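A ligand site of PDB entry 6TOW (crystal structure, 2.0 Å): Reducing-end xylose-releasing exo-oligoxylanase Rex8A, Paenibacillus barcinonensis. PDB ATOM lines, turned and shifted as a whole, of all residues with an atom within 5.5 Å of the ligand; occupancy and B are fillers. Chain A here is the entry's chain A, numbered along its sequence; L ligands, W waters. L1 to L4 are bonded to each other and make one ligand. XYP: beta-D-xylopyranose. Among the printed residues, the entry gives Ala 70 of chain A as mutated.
OD2 of Asp 128 lies within salt-bridge range of NH1 of Arg 268 (3.6 Å). NE of Arg 268 is in hydrogen-bond range of OH of Tyr 361, 3.1 Å away. The guanidinium group of Arg 268 sits at hydrogen-bond distance from the side-chain hydroxyl of Ser 196, at 3.1 Å. NE of Arg 68 lies within salt-bridge range of OD2 of Asp 61, at 3.0 Å. OD2 of Asp 61 is in hydrogen-bond range of ND2 of Asn 64 (2.7 Å). NE2 of His 256 is in hydrogen-bond range of OH of Tyr 243, 3.0 Å away. The backbone carbonyl oxygen of Trp 112 is in hydrogen-bond range of the backbone NH of Ser 69. OH of Tyr 361 lies within hydrogen-bond range of O of Ser 264 (2.7 Å).
OD2 of Asp 128 sits at hydrogen-bond distance from O2 of XYP L2 (2.5 Å). An oxygen (O1) of XYP L1 sits at hydrogen-bond distance from a ring nitrogen (NE2) of His 321 (2.8 Å). An oxygen (O2) of XYP L2 is in hydrogen-bond range of the guanidinium group (NH1) of Arg 268 (2.9 Å). OD2 of Asp 61 lies within hydrogen-bond range of O2 of XYP L1 (3.0 Å). O3 of XYP L1 is in hydrogen-bond range of NH1 of Arg 68, at 3.0 Å. An oxygen (O3) of XYP L3 lies within hydrogen-bond range of a ring nitrogen (NE2) of His 256 (3.4 Å).
ND2 of Asn 64 touches O2 of XYP L1 (3.7 Å). CB of Ala 70 touches O3 of XYP L2, at 3.5 Å. NE1 of Trp 112 touches O4 of XYP L3, at 3.6 Å. Gly 124 touches the ligand. O of Pro 125 touches C5 of XYP L3, at 3.7 Å. Ala 126 touches the ligand. CZ of Phe 186 touches O3 of XYP L3, 3.7 Å away. CD1 of Ile 187 touches C3 of XYP L4, at 3.9 Å. OH of Tyr 197 touches O4 of XYP L2, at 3.5 Å. Ser 264 touches the ligand. Asp 265 touches the ligand. Leu 320 touches the ligand. CE2 of Tyr 360 touches O2 of XYP L1 (3.8 Å). Tyr 361 touches the ligand. Hydrophobic or aromatic side chains within 4 Å of the ligand: Ala 70, Trp 112, Ala 126, Phe 186, Ile 187, Tyr 197, His 256, Leu 320, His 321, Tyr 360 and Tyr 361. Of the 28 residues printed, 20 come within 4 Å of the ligand. The nearest printed residue that does not touch the ligand is Tyr 243 (4.1 Å).
Water W7 lies within hydrogen-bond range of an oxygen (O2) of XYP L4 (2.5 Å) and the backbone carbonyl oxygen (O) of Pro 125 (2.5 Å). Water W9 lies within hydrogen-bond range of an oxygen (O2) of XYP L4 (2.6 Å) and the backbone NH of Gly 124 (3.0 Å). Water W1 lies within hydrogen-bond range of OH of Tyr 197 (2.6 Å), O of Phe 186 (2.7 Å) and O5 of XYP L3 (2.8 Å). Water W3 bridges the side-chain hydroxyl (OH) of Tyr 243 and an oxygen (O2) of XYP L3. Water W6 lies within hydrogen-bond range of the side-chain hydroxyl of Ser 264 and an oxygen (O5) of XYP L1. Water W10 lies within hydrogen-bond range of OD2 of Asp 265, OH of Tyr 197 and O4 of XYP L2.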
ATOM      1  N   ASP A  61      23.595  36.073 -21.235  1.00  0.00           N
ATOM      2  CA  ASP A  61      23.455  35.334 -22.515  1.00  0.00           C
ATOM      3  C   ASP A  61      22.135  35.805 -23.132  1.00  0.00           C
ATOM      4  O   ASP A  61      21.071  35.304 -22.736  1.00  0.00           O
ATOM      5  CB  ASP A  61      23.561  33.814 -22.365  1.00  0.00           C
ATOM      6  CG  ASP A  61      23.491  33.066 -23.686  1.00  0.00           C
ATOM      7  OD1 ASP A  61      23.019  33.664 -24.695  1.00  0.00           O
ATOM      8  OD2 ASP A  61      23.885  31.898 -23.708  1.00  0.00           O
ATOM      9  N   ASN A  64      19.910  33.083 -24.982  1.00  0.00           N
ATOM     10  CA  ASN A  64      19.271  32.030 -24.137  1.00  0.00           C
ATOM     11  C   ASN A  64      18.531  32.656 -22.945  1.00  0.00           C
ATOM     12  O   ASN A  64      17.999  31.877 -22.129  1.00  0.00           O
ATOM     13  CB  ASN A  64      20.317  31.010 -23.668  1.00  0.00           C
ATOM     14  CG  ASN A  64      20.896  30.217 -24.830  1.00  0.00           C
ATOM     15  OD1 ASN A  64      20.190  29.417 -25.420  1.00  0.00           O
ATOM     16  ND2 ASN A  64      22.165  30.433 -25.159  1.00  0.00           N
ATOM     17  N   ARG A  68      25.309  32.638 -17.394  1.00  0.00           N
ATOM     18  CA  ARG A  68      26.152  31.413 -17.469  1.00  0.00           C
ATOM     19  C   ARG A  68      27.456  31.644 -16.701  1.00  0.00           C
ATOM     20  O   ARG A  68      27.968  32.782 -16.732  1.00  0.00           O
ATOM     21  CB  ARG A  68      26.407  31.061 -18.928  1.00  0.00           C
ATOM     22  CG  ARG A  68      25.234  30.345 -19.564  1.00  0.00           C
ATOM     23  CD  ARG A  68      25.096  30.415 -21.076  1.00  0.00           C
ATOM     24  NE  ARG A  68      23.730  29.963 -21.360  1.00  0.00           N
ATOM     25  CZ  ARG A  68      23.379  28.948 -22.164  1.00  0.00           C
ATOM     26  NH1 ARG A  68      24.270  28.265 -22.850  1.00  0.00           N
ATOM     27  NH2 ARG A  68      22.102  28.623 -22.255  1.00  0.00           N
ATOM     28  N   SER A  69      27.953  30.595 -16.061  1.00  0.00           N
ATOM     29  CA  SER A  69      29.239  30.612 -15.322  1.00  0.00           C
ATOM     30  C   SER A  69      30.365  31.017 -16.292  1.00  0.00           C
ATOM     31  O   SER A  69      31.220  31.814 -15.893  1.00  0.00           O
ATOM     32  CB  SER A  69      29.517  29.300 -14.630  1.00  0.00           C
ATOM     33  OG  SER A  69      29.532  28.221 -15.550  1.00  0.00           O
ATOM     34  N   ALA A  70      30.329  30.547 -17.535  1.00  0.00           N
ATOM     35  CA  ALA A  70      31.339  30.891 -18.565  1.00  0.00           C
ATOM     36  C   ALA A  70      31.265  32.401 -18.828  1.00  0.00           C
ATOM     37  O   ALA A  70      32.324  33.047 -18.846  1.00  0.00           O
ATOM     38  CB  ALA A  70      31.118  30.074 -19.817  1.00  0.00           C
ATOM     39  N   TYR A  74      34.060  35.147 -17.871  1.00  0.00           N
ATOM     40  CA  TYR A  74      34.591  35.974 -18.979  1.00  0.00           C
ATOM     41  C   TYR A  74      34.541  37.457 -18.590  1.00  0.00           C
ATOM     42  O   TYR A  74      35.533  38.187 -18.825  1.00  0.00           O
ATOM     43  CB  TYR A  74      33.767  35.836 -20.259  1.00  0.00           C
ATOM     44  CG  TYR A  74      33.953  34.571 -21.051  1.00  0.00           C
ATOM     45  CD1 TYR A  74      34.994  33.694 -20.811  1.00  0.00           C
ATOM     46  CD2 TYR A  74      33.048  34.253 -22.072  1.00  0.00           C
ATOM     47  CE1 TYR A  74      35.152  32.545 -21.574  1.00  0.00           C
ATOM     48  CE2 TYR A  74      33.210  33.120 -22.851  1.00  0.00           C
ATOM     49  CZ  TYR A  74      34.259  32.266 -22.605  1.00  0.00           C
ATOM     50  OH  TYR A  74      34.391  31.117 -23.322  1.00  0.00           O
ATOM     51  N   TYR A 106      28.700  19.128  -5.491  1.00  0.00           N
ATOM     52  CA  TYR A 106      29.242  20.252  -6.303  1.00  0.00           C
ATOM     53  C   TYR A 106      29.763  21.408  -5.444  1.00  0.00           C
ATOM     54  O   TYR A 106      29.957  22.503  -6.000  1.00  0.00           O
ATOM     55  CB  TYR A 106      28.188  20.818  -7.266  1.00  0.00           C
ATOM     56  CG  TYR A 106      27.600  19.825  -8.229  1.00  0.00           C
ATOM     57  CD1 TYR A 106      28.431  19.009  -8.979  1.00  0.00           C
ATOM     58  CD2 TYR A 106      26.236  19.724  -8.425  1.00  0.00           C
ATOM     59  CE1 TYR A 106      27.910  18.092  -9.883  1.00  0.00           C
ATOM     60  CE2 TYR A 106      25.698  18.811  -9.317  1.00  0.00           C
ATOM     61  CZ  TYR A 106      26.545  18.004 -10.054  1.00  0.00           C
ATOM     62  OH  TYR A 106      26.053  17.098 -10.955  1.00  0.00           O
ATOM     63  N   TRP A 112      25.832  26.038 -13.468  1.00  0.00           N
ATOM     64  CA  TRP A 112      26.379  26.572 -14.754  1.00  0.00           C
ATOM     65  C   TRP A 112      25.480  27.695 -15.277  1.00  0.00           C
ATOM     66  O   TRP A 112      26.006  28.533 -16.028  1.00  0.00           O
ATOM     67  CB  TRP A 112      26.618  25.482 -15.796  1.00  0.00           C
ATOM     68  CG  TRP A 112      25.412  24.937 -16.502  1.00  0.00           C
ATOM     69  CD1 TRP A 112      24.647  23.871 -16.127  1.00  0.00           C
ATOM     70  CD2 TRP A 112      24.903  25.356 -17.778  1.00  0.00           C
ATOM     71  NE1 TRP A 112      23.678  23.617 -17.063  1.00  0.00           N
ATOM     72  CE2 TRP A 112      23.810  24.521 -18.094  1.00  0.00           C
ATOM     73  CE3 TRP A 112      25.252  26.374 -18.678  1.00  0.00           C
ATOM     74  CZ2 TRP A 112      23.054  24.691 -19.248  1.00  0.00           C
ATOM     75  CZ3 TRP A 112      24.502  26.550 -19.811  1.00  0.00           C
ATOM     76  CH2 TRP A 112      23.417  25.714 -20.094  1.00  0.00           C
ATOM     77  N   SER A 122      20.026  25.022 -13.393  1.00  0.00           N
ATOM     78  CA  SER A 122      20.636  23.675 -13.296  1.00  0.00           C
ATOM     79  C   SER A 122      21.648  23.677 -12.156  1.00  0.00           C
ATOM     80  O   SER A 122      22.358  24.663 -11.981  1.00  0.00           O
ATOM     81  CB  SER A 122      21.311  23.253 -14.558  1.00  0.00           C
ATOM     82  OG  SER A 122      20.445  23.261 -15.659  1.00  0.00           O
ATOM     83  N   GLY A 124      24.291  21.412 -11.951  1.00  0.00           N
ATOM     84  CA  GLY A 124      25.577  20.944 -12.495  1.00  0.00           C
ATOM     85  C   GLY A 124      26.479  22.111 -12.916  1.00  0.00           C
ATOM     86  O   GLY A 124      25.996  23.150 -13.377  1.00  0.00           O
ATOM     87  N   PRO A 125      27.819  21.979 -12.819  1.00  0.00           N
ATOM     88  CA  PRO A 125      28.743  23.020 -13.240  1.00  0.00           C
ATOM     89  C   PRO A 125      29.192  22.867 -14.704  1.00  0.00           C
ATOM     90  O   PRO A 125      28.912  21.850 -15.348  1.00  0.00           O
ATOM     91  CB  PRO A 125      29.927  22.780 -12.299  1.00  0.00           C
ATOM     92  CG  PRO A 125      29.971  21.275 -12.166  1.00  0.00           C
ATOM     93  CD  PRO A 125      28.533  20.802 -12.291  1.00  0.00           C
ATOM     94  N   ALA A 126      29.895  23.890 -15.194  1.00  0.00           N
ATOM     95  CA  ALA A 126      30.582  23.873 -16.505  1.00  0.00           C
ATOM     96  C   ALA A 126      32.049  24.207 -16.270  1.00  0.00           C
ATOM     97  O   ALA A 126      32.354  25.367 -16.004  1.00  0.00           O
ATOM     98  CB  ALA A 126      29.915  24.847 -17.428  1.00  0.00           C
ATOM     99  N   ASP A 128      34.697  25.025 -17.745  1.00  0.00           N
ATOM    100  CA  ASP A 128      35.354  26.209 -18.370  1.00  0.00           C
ATOM    101  C   ASP A 128      35.067  27.464 -17.537  1.00  0.00           C
ATOM    102  O   ASP A 128      35.893  28.401 -17.563  1.00  0.00           O
ATOM    103  CB  ASP A 128      35.019  26.365 -19.859  1.00  0.00           C
ATOM    104  CG  ASP A 128      33.547  26.538 -20.184  1.00  0.00           C
ATOM    105  OD1 ASP A 128      32.718  25.892 -19.498  1.00  0.00           O
ATOM    106  OD2 ASP A 128      33.257  27.279 -21.124  1.00  0.00           O
ATOM    107  N   GLY A 129      33.940  27.498 -16.822  1.00  0.00           N
ATOM    108  CA  GLY A 129      33.614  28.599 -15.891  1.00  0.00           C
ATOM    109  C   GLY A 129      34.617  28.627 -14.732  1.00  0.00           C
ATOM    110  O   GLY A 129      35.231  29.696 -14.498  1.00  0.00           O
ATOM    111  N   PHE A 186      34.505  17.557 -19.891  1.00  0.00           N
ATOM    112  CA  PHE A 186      33.295  18.301 -20.300  1.00  0.00           C
ATOM    113  C   PHE A 186      32.451  18.637 -19.056  1.00  0.00           C
ATOM    114  O   PHE A 186      32.078  19.808 -18.925  1.00  0.00           O
ATOM    115  CB  PHE A 186      32.511  17.486 -21.333  1.00  0.00           C
ATOM    116  CG  PHE A 186      31.119  18.005 -21.543  1.00  0.00           C
ATOM    117  CD1 PHE A 186      30.898  19.312 -21.963  1.00  0.00           C
ATOM    118  CD2 PHE A 186      30.009  17.200 -21.291  1.00  0.00           C
ATOM    119  CE1 PHE A 186      29.616  19.807 -22.117  1.00  0.00           C
ATOM    120  CE2 PHE A 186      28.727  17.695 -21.445  1.00  0.00           C
ATOM    121  CZ  PHE A 186      28.530  19.005 -21.858  1.00  0.00           C
ATOM    122  N   ILE A 187      32.096  17.638 -18.229  1.00  0.00           N
ATOM    123  CA  ILE A 187      31.469  17.825 -16.882  1.00  0.00           C
ATOM    124  C   ILE A 187      32.054  16.768 -15.943  1.00  0.00           C
ATOM    125  O   ILE A 187      32.619  15.766 -16.380  1.00  0.00           O
ATOM    126  CB  ILE A 187      29.921  17.752 -16.899  1.00  0.00           C
ATOM    127  CG1 ILE A 187      29.408  16.373 -17.301  1.00  0.00           C
ATOM    128  CG2 ILE A 187      29.330  18.869 -17.772  1.00  0.00           C
ATOM    129  CD1 ILE A 187      27.889  16.246 -17.212  1.00  0.00           C
ATOM    130  N   LEU A 190      31.205  12.791 -16.687  1.00  0.00           N
ATOM    131  CA  LEU A 190      31.359  12.116 -18.006  1.00  0.00           C
ATOM    132  C   LEU A 190      32.836  11.962 -18.367  1.00  0.00           C
ATOM    133  O   LEU A 190      33.629  12.870 -18.152  1.00  0.00           O
ATOM    134  CB  LEU A 190      30.575  12.890 -19.071  1.00  0.00           C
ATOM    135  CG  LEU A 190      29.048  12.885 -18.893  1.00  0.00           C
ATOM    136  CD1 LEU A 190      28.366  13.779 -19.927  1.00  0.00           C
ATOM    137  CD2 LEU A 190      28.465  11.468 -18.986  1.00  0.00           C
ATOM    138  N   SER A 196      37.915  23.273 -26.498  1.00  0.00           N
ATOM    139  CA  SER A 196      37.833  24.719 -26.147  1.00  0.00           C
ATOM    140  C   SER A 196      38.085  24.964 -24.644  1.00  0.00           C
ATOM    141  O   SER A 196      38.392  26.126 -24.292  1.00  0.00           O
ATOM    142  CB  SER A 196      36.518  25.335 -26.583  1.00  0.00           C
ATOM    143  OG  SER A 196      35.460  24.907 -25.765  1.00  0.00           O
ATOM    144  N   TYR A 197      37.948  23.957 -23.783  1.00  0.00           N
ATOM    145  CA  TYR A 197      38.120  24.094 -22.317  1.00  0.00           C
ATOM    146  C   TYR A 197      39.604  23.975 -21.915  1.00  0.00           C
ATOM    147  O   TYR A 197      39.921  24.246 -20.754  1.00  0.00           O
ATOM    148  CB  TYR A 197      37.348  23.015 -21.557  1.00  0.00           C
ATOM    149  CG  TYR A 197      35.844  23.078 -21.601  1.00  0.00           C
ATOM    150  CD1 TYR A 197      35.143  23.894 -22.480  1.00  0.00           C
ATOM    151  CD2 TYR A 197      35.112  22.296 -20.719  1.00  0.00           C
ATOM    152  CE1 TYR A 197      33.744  23.927 -22.490  1.00  0.00           C
ATOM    153  CE2 TYR A 197      33.720  22.321 -20.709  1.00  0.00           C
ATOM    154  CZ  TYR A 197      33.037  23.127 -21.613  1.00  0.00           C
ATOM    155  OH  TYR A 197      31.676  23.117 -21.562  1.00  0.00           O
ATOM    156  N   TYR A 243      32.917  18.706 -28.824  1.00  0.00           N
ATOM    157  CA  TYR A 243      33.171  17.667 -27.770  1.00  0.00           C
ATOM    158  C   TYR A 243      34.058  16.575 -28.351  1.00  0.00           C
ATOM    159  O   TYR A 243      33.835  16.138 -29.514  1.00  0.00           O
ATOM    160  CB  TYR A 243      31.903  16.992 -27.224  1.00  0.00           C
ATOM    161  CG  TYR A 243      30.856  17.840 -26.536  1.00  0.00           C
ATOM    162  CD1 TYR A 243      30.993  19.212 -26.363  1.00  0.00           C
ATOM    163  CD2 TYR A 243      29.682  17.257 -26.104  1.00  0.00           C
ATOM    164  CE1 TYR A 243      29.998  19.958 -25.750  1.00  0.00           C
ATOM    165  CE2 TYR A 243      28.683  17.987 -25.475  1.00  0.00           C
ATOM    166  CZ  TYR A 243      28.840  19.348 -25.303  1.00  0.00           C
ATOM    167  OH  TYR A 243      27.857  20.081 -24.699  1.00  0.00           O
ATOM    168  N   HIS A 256      21.521  15.939 -25.870  1.00  0.00           N
ATOM    169  CA  HIS A 256      21.193  17.390 -25.986  1.00  0.00           C
ATOM    170  C   HIS A 256      21.765  17.993 -27.282  1.00  0.00           C
ATOM    171  O   HIS A 256      21.537  19.200 -27.503  1.00  0.00           O
ATOM    172  CB  HIS A 256      21.632  18.150 -24.723  1.00  0.00           C
ATOM    173  CG  HIS A 256      23.114  18.214 -24.490  1.00  0.00           C
ATOM    174  ND1 HIS A 256      23.840  17.143 -24.013  1.00  0.00           N
ATOM    175  CD2 HIS A 256      23.998  19.239 -24.652  1.00  0.00           C
ATOM    176  CE1 HIS A 256      25.108  17.493 -23.904  1.00  0.00           C
ATOM    177  NE2 HIS A 256      25.231  18.773 -24.284  1.00  0.00           N
ATOM    178  N   SER A 264      30.169  26.554 -32.420  1.00  0.00           N
ATOM    179  CA  SER A 264      30.326  27.605 -31.379  1.00  0.00           C
ATOM    180  C   SER A 264      31.500  27.356 -30.418  1.00  0.00           C
ATOM    181  O   SER A 264      32.404  28.218 -30.349  1.00  0.00           O
ATOM    182  CB  SER A 264      29.009  27.793 -30.674  1.00  0.00           C
ATOM    183  OG  SER A 264      27.987  28.078 -31.640  1.00  0.00           O
ATOM    184  N   ASP A 265      31.490  26.251 -29.663  1.00  0.00           N
ATOM    185  CA  ASP A 265      32.517  25.996 -28.601  1.00  0.00           C
ATOM    186  C   ASP A 265      33.924  26.022 -29.219  1.00  0.00           C
ATOM    187  O   ASP A 265      34.793  26.651 -28.635  1.00  0.00           O
ATOM    188  CB  ASP A 265      32.347  24.620 -27.954  1.00  0.00           C
ATOM    189  CG  ASP A 265      31.305  24.568 -26.872  1.00  0.00           C
ATOM    190  OD1 ASP A 265      30.340  25.317 -26.976  1.00  0.00           O
ATOM    191  OD2 ASP A 265      31.490  23.798 -25.913  1.00  0.00           O
ATOM    192  N   ARG A 268      36.928  28.818 -29.927  1.00  0.00           N
ATOM    193  CA  ARG A 268      37.859  29.330 -28.883  1.00  0.00           C
ATOM    194  C   ARG A 268      39.206  28.590 -28.984  1.00  0.00           C
ATOM    195  O   ARG A 268      40.208  29.152 -28.513  1.00  0.00           O
ATOM    196  CB  ARG A 268      37.214  29.191 -27.510  1.00  0.00           C
ATOM    197  CG  ARG A 268      35.974  30.063 -27.344  1.00  0.00           C
ATOM    198  CD  ARG A 268      35.208  29.751 -26.087  1.00  0.00           C
ATOM    199  NE  ARG A 268      34.585  28.430 -26.102  1.00  0.00           N
ATOM    200  CZ  ARG A 268      33.615  28.048 -25.266  1.00  0.00           C
ATOM    201  NH1 ARG A 268      33.150  28.881 -24.357  1.00  0.00           N
ATOM    202  NH2 ARG A 268      33.124  26.819 -25.323  1.00  0.00           N
ATOM    203  N   LEU A 320      26.033  30.025 -36.153  1.00  0.00           N
ATOM    204  CA  LEU A 320      25.150  30.832 -35.275  1.00  0.00           C
ATOM    205  C   LEU A 320      25.885  32.095 -34.825  1.00  0.00           C
ATOM    206  O   LEU A 320      25.230  33.155 -34.688  1.00  0.00           O
ATOM    207  CB  LEU A 320      24.724  29.990 -34.070  1.00  0.00           C
ATOM    208  CG  LEU A 320      23.976  30.728 -32.965  1.00  0.00           C
ATOM    209  CD1 LEU A 320      22.728  31.364 -33.543  1.00  0.00           C
ATOM    210  CD2 LEU A 320      23.602  29.785 -31.835  1.00  0.00           C
ATOM    211  N   HIS A 321      27.192  31.991 -34.578  1.00  0.00           N
ATOM    212  CA  HIS A 321      28.032  33.100 -34.066  1.00  0.00           C
ATOM    213  C   HIS A 321      29.181  33.380 -35.036  1.00  0.00           C
ATOM    214  O   HIS A 321      30.344  33.110 -34.735  1.00  0.00           O
ATOM    215  CB  HIS A 321      28.517  32.769 -32.659  1.00  0.00           C
ATOM    216  CG  HIS A 321      27.418  32.468 -31.701  1.00  0.00           C
ATOM    217  ND1 HIS A 321      26.555  33.436 -31.248  1.00  0.00           N
ATOM    218  CD2 HIS A 321      27.035  31.316 -31.099  1.00  0.00           C
ATOM    219  CE1 HIS A 321      25.676  32.882 -30.450  1.00  0.00           C
ATOM    220  NE2 HIS A 321      25.963  31.604 -30.335  1.00  0.00           N
ATOM    221  N   TYR A 360      25.591  37.948 -27.613  1.00  0.00           N
ATOM    222  CA  TYR A 360      26.388  37.714 -26.388  1.00  0.00           C
ATOM    223  C   TYR A 360      27.684  36.947 -26.713  1.00  0.00           C
ATOM    224  O   TYR A 360      28.755  37.440 -26.356  1.00  0.00           O
ATOM    225  CB  TYR A 360      25.571  37.014 -25.303  1.00  0.00           C
ATOM    226  CG  TYR A 360      26.347  36.139 -24.354  1.00  0.00           C
ATOM    227  CD1 TYR A 360      26.989  36.656 -23.226  1.00  0.00           C
ATOM    228  CD2 TYR A 360      26.400  34.772 -24.548  1.00  0.00           C
ATOM    229  CE1 TYR A 360      27.692  35.826 -22.349  1.00  0.00           C
ATOM    230  CE2 TYR A 360      27.086  33.933 -23.683  1.00  0.00           C
ATOM    231  CZ  TYR A 360      27.732  34.460 -22.583  1.00  0.00           C
ATOM    232  OH  TYR A 360      28.405  33.580 -21.769  1.00  0.00           O
ATOM    233  N   TYR A 361      27.591  35.761 -27.331  1.00  0.00           N
ATOM    234  CA  TYR A 361      28.759  34.859 -27.516  1.00  0.00           C
ATOM    235  C   TYR A 361      29.748  35.483 -28.503  1.00  0.00           C
ATOM    236  O   TYR A 361      30.962  35.520 -28.201  1.00  0.00           O
ATOM    237  CB  TYR A 361      28.333  33.467 -27.972  1.00  0.00           C
ATOM    238  CG  TYR A 361      29.438  32.437 -27.977  1.00  0.00           C
ATOM    239  CD1 TYR A 361      29.989  31.945 -26.806  1.00  0.00           C
ATOM    240  CD2 TYR A 361      29.977  31.963 -29.171  1.00  0.00           C
ATOM    241  CE1 TYR A 361      30.994  31.001 -26.801  1.00  0.00           C
ATOM    242  CE2 TYR A 361      30.972  31.004 -29.183  1.00  0.00           C
ATOM    243  CZ  TYR A 361      31.493  30.522 -28.001  1.00  0.00           C
ATOM    244  OH  TYR A 361      32.485  29.585 -28.024  1.00  0.00           O
HETATM  245  O1  XYP L   1      25.321  29.686 -28.458  1.00  0.00           O
HETATM  246  C1  XYP L   1      26.467  29.579 -27.544  1.00  0.00           C
HETATM  247  C2  XYP L   1      26.004  29.918 -26.101  1.00  0.00           C
HETATM  248  C3  XYP L   1      27.159  29.764 -25.117  1.00  0.00           C
HETATM  249  C4  XYP L   1      27.953  28.410 -25.287  1.00  0.00           C
HETATM  250  C5  XYP L   1      28.407  28.263 -26.731  1.00  0.00           C
HETATM  251  O2  XYP L   1      25.597  31.310 -26.040  1.00  0.00           O
HETATM  252  O3  XYP L   1      26.636  29.958 -23.761  1.00  0.00           O
HETATM  253  O4  XYP L   1      29.120  28.332 -24.340  1.00  0.00           O
HETATM  254  O5  XYP L   1      27.141  28.291 -27.562  1.00  0.00           O
HETATM  255  C1  XYP L   2      29.015  27.190 -23.436  1.00  0.00           C
HETATM  256  C2  XYP L   2      30.040  27.304 -22.334  1.00  0.00           C
HETATM  257  C3  XYP L   2      29.761  26.192 -21.285  1.00  0.00           C
HETATM  258  C4  XYP L   2      28.277  25.642 -21.208  1.00  0.00           C
HETATM  259  C5  XYP L   2      27.378  25.952 -22.395  1.00  0.00           C
HETATM  260  O2  XYP L   2      31.422  27.119 -22.849  1.00  0.00           O
HETATM  261  O3  XYP L   2      30.127  26.722 -20.045  1.00  0.00           O
HETATM  262  O4  XYP L   2      28.335  24.182 -21.175  1.00  0.00           O
HETATM  263  O5  XYP L   2      27.709  27.230 -22.847  1.00  0.00           O
HETATM  264  C1  XYP L   3      27.287  23.519 -20.470  1.00  0.00           C
HETATM  265  C2  XYP L   3      26.660  22.451 -21.375  1.00  0.00           C
HETATM  266  C3  XYP L   3      25.672  21.634 -20.585  1.00  0.00           C
HETATM  267  C4  XYP L   3      26.310  21.125 -19.316  1.00  0.00           C
HETATM  268  C5  XYP L   3      27.093  22.178 -18.518  1.00  0.00           C
HETATM  269  O2  XYP L   3      25.996  23.005 -22.526  1.00  0.00           O
HETATM  270  O3  XYP L   3      25.219  20.474 -21.369  1.00  0.00           O
HETATM  271  O4  XYP L   3      25.231  20.754 -18.535  1.00  0.00           O
HETATM  272  O5  XYP L   3      27.995  22.883 -19.388  1.00  0.00           O
HETATM  273  C1  XYP L   4      25.130  19.346 -18.343  1.00  0.00           C
HETATM  274  C2  XYP L   4      24.189  19.101 -17.155  1.00  0.00           C
HETATM  275  C3  XYP L   4      24.237  17.609 -16.886  1.00  0.00           C
HETATM  276  C4  XYP L   4      23.597  16.919 -18.111  1.00  0.00           C
HETATM  277  C5  XYP L   4      24.305  17.292 -19.439  1.00  0.00           C
HETATM  278  O2  XYP L   4      24.498  19.978 -15.985  1.00  0.00           O
HETATM  279  O3  XYP L   4      23.482  17.282 -15.699  1.00  0.00           O
HETATM  280  O4  XYP L   4      23.682  15.516 -17.924  1.00  0.00           O
HETATM  281  O5  XYP L   4      24.578  18.739 -19.551  1.00  0.00           O
HETATM  282  O   HOH W   1      30.615  22.044 -19.482  1.00  0.00           O
HETATM  283  O   HOH W   2      23.626  32.825 -27.102  1.00  0.00           O
HETATM  284  O   HOH W   3      27.656  22.709 -24.727  1.00  0.00           O
HETATM  285  O   HOH W   4      22.830  28.802 -27.695  1.00  0.00           O
HETATM  286  O   HOH W   5      28.536  31.160 -22.515  1.00  0.00           O
HETATM  287  O   HOH W   6      26.023  27.148 -30.107  1.00  0.00           O
HETATM  288  O   HOH W   7      26.920  20.321 -15.451  1.00  0.00           O
HETATM  289  O   HOH W   8      28.734  28.224 -18.104  1.00  0.00           O
HETATM  290  O   HOH W   9      22.742  19.812 -14.008  1.00  0.00           O
HETATM  291  O   HOH W  10      30.198  23.520 -23.797  1.00  0.00           O
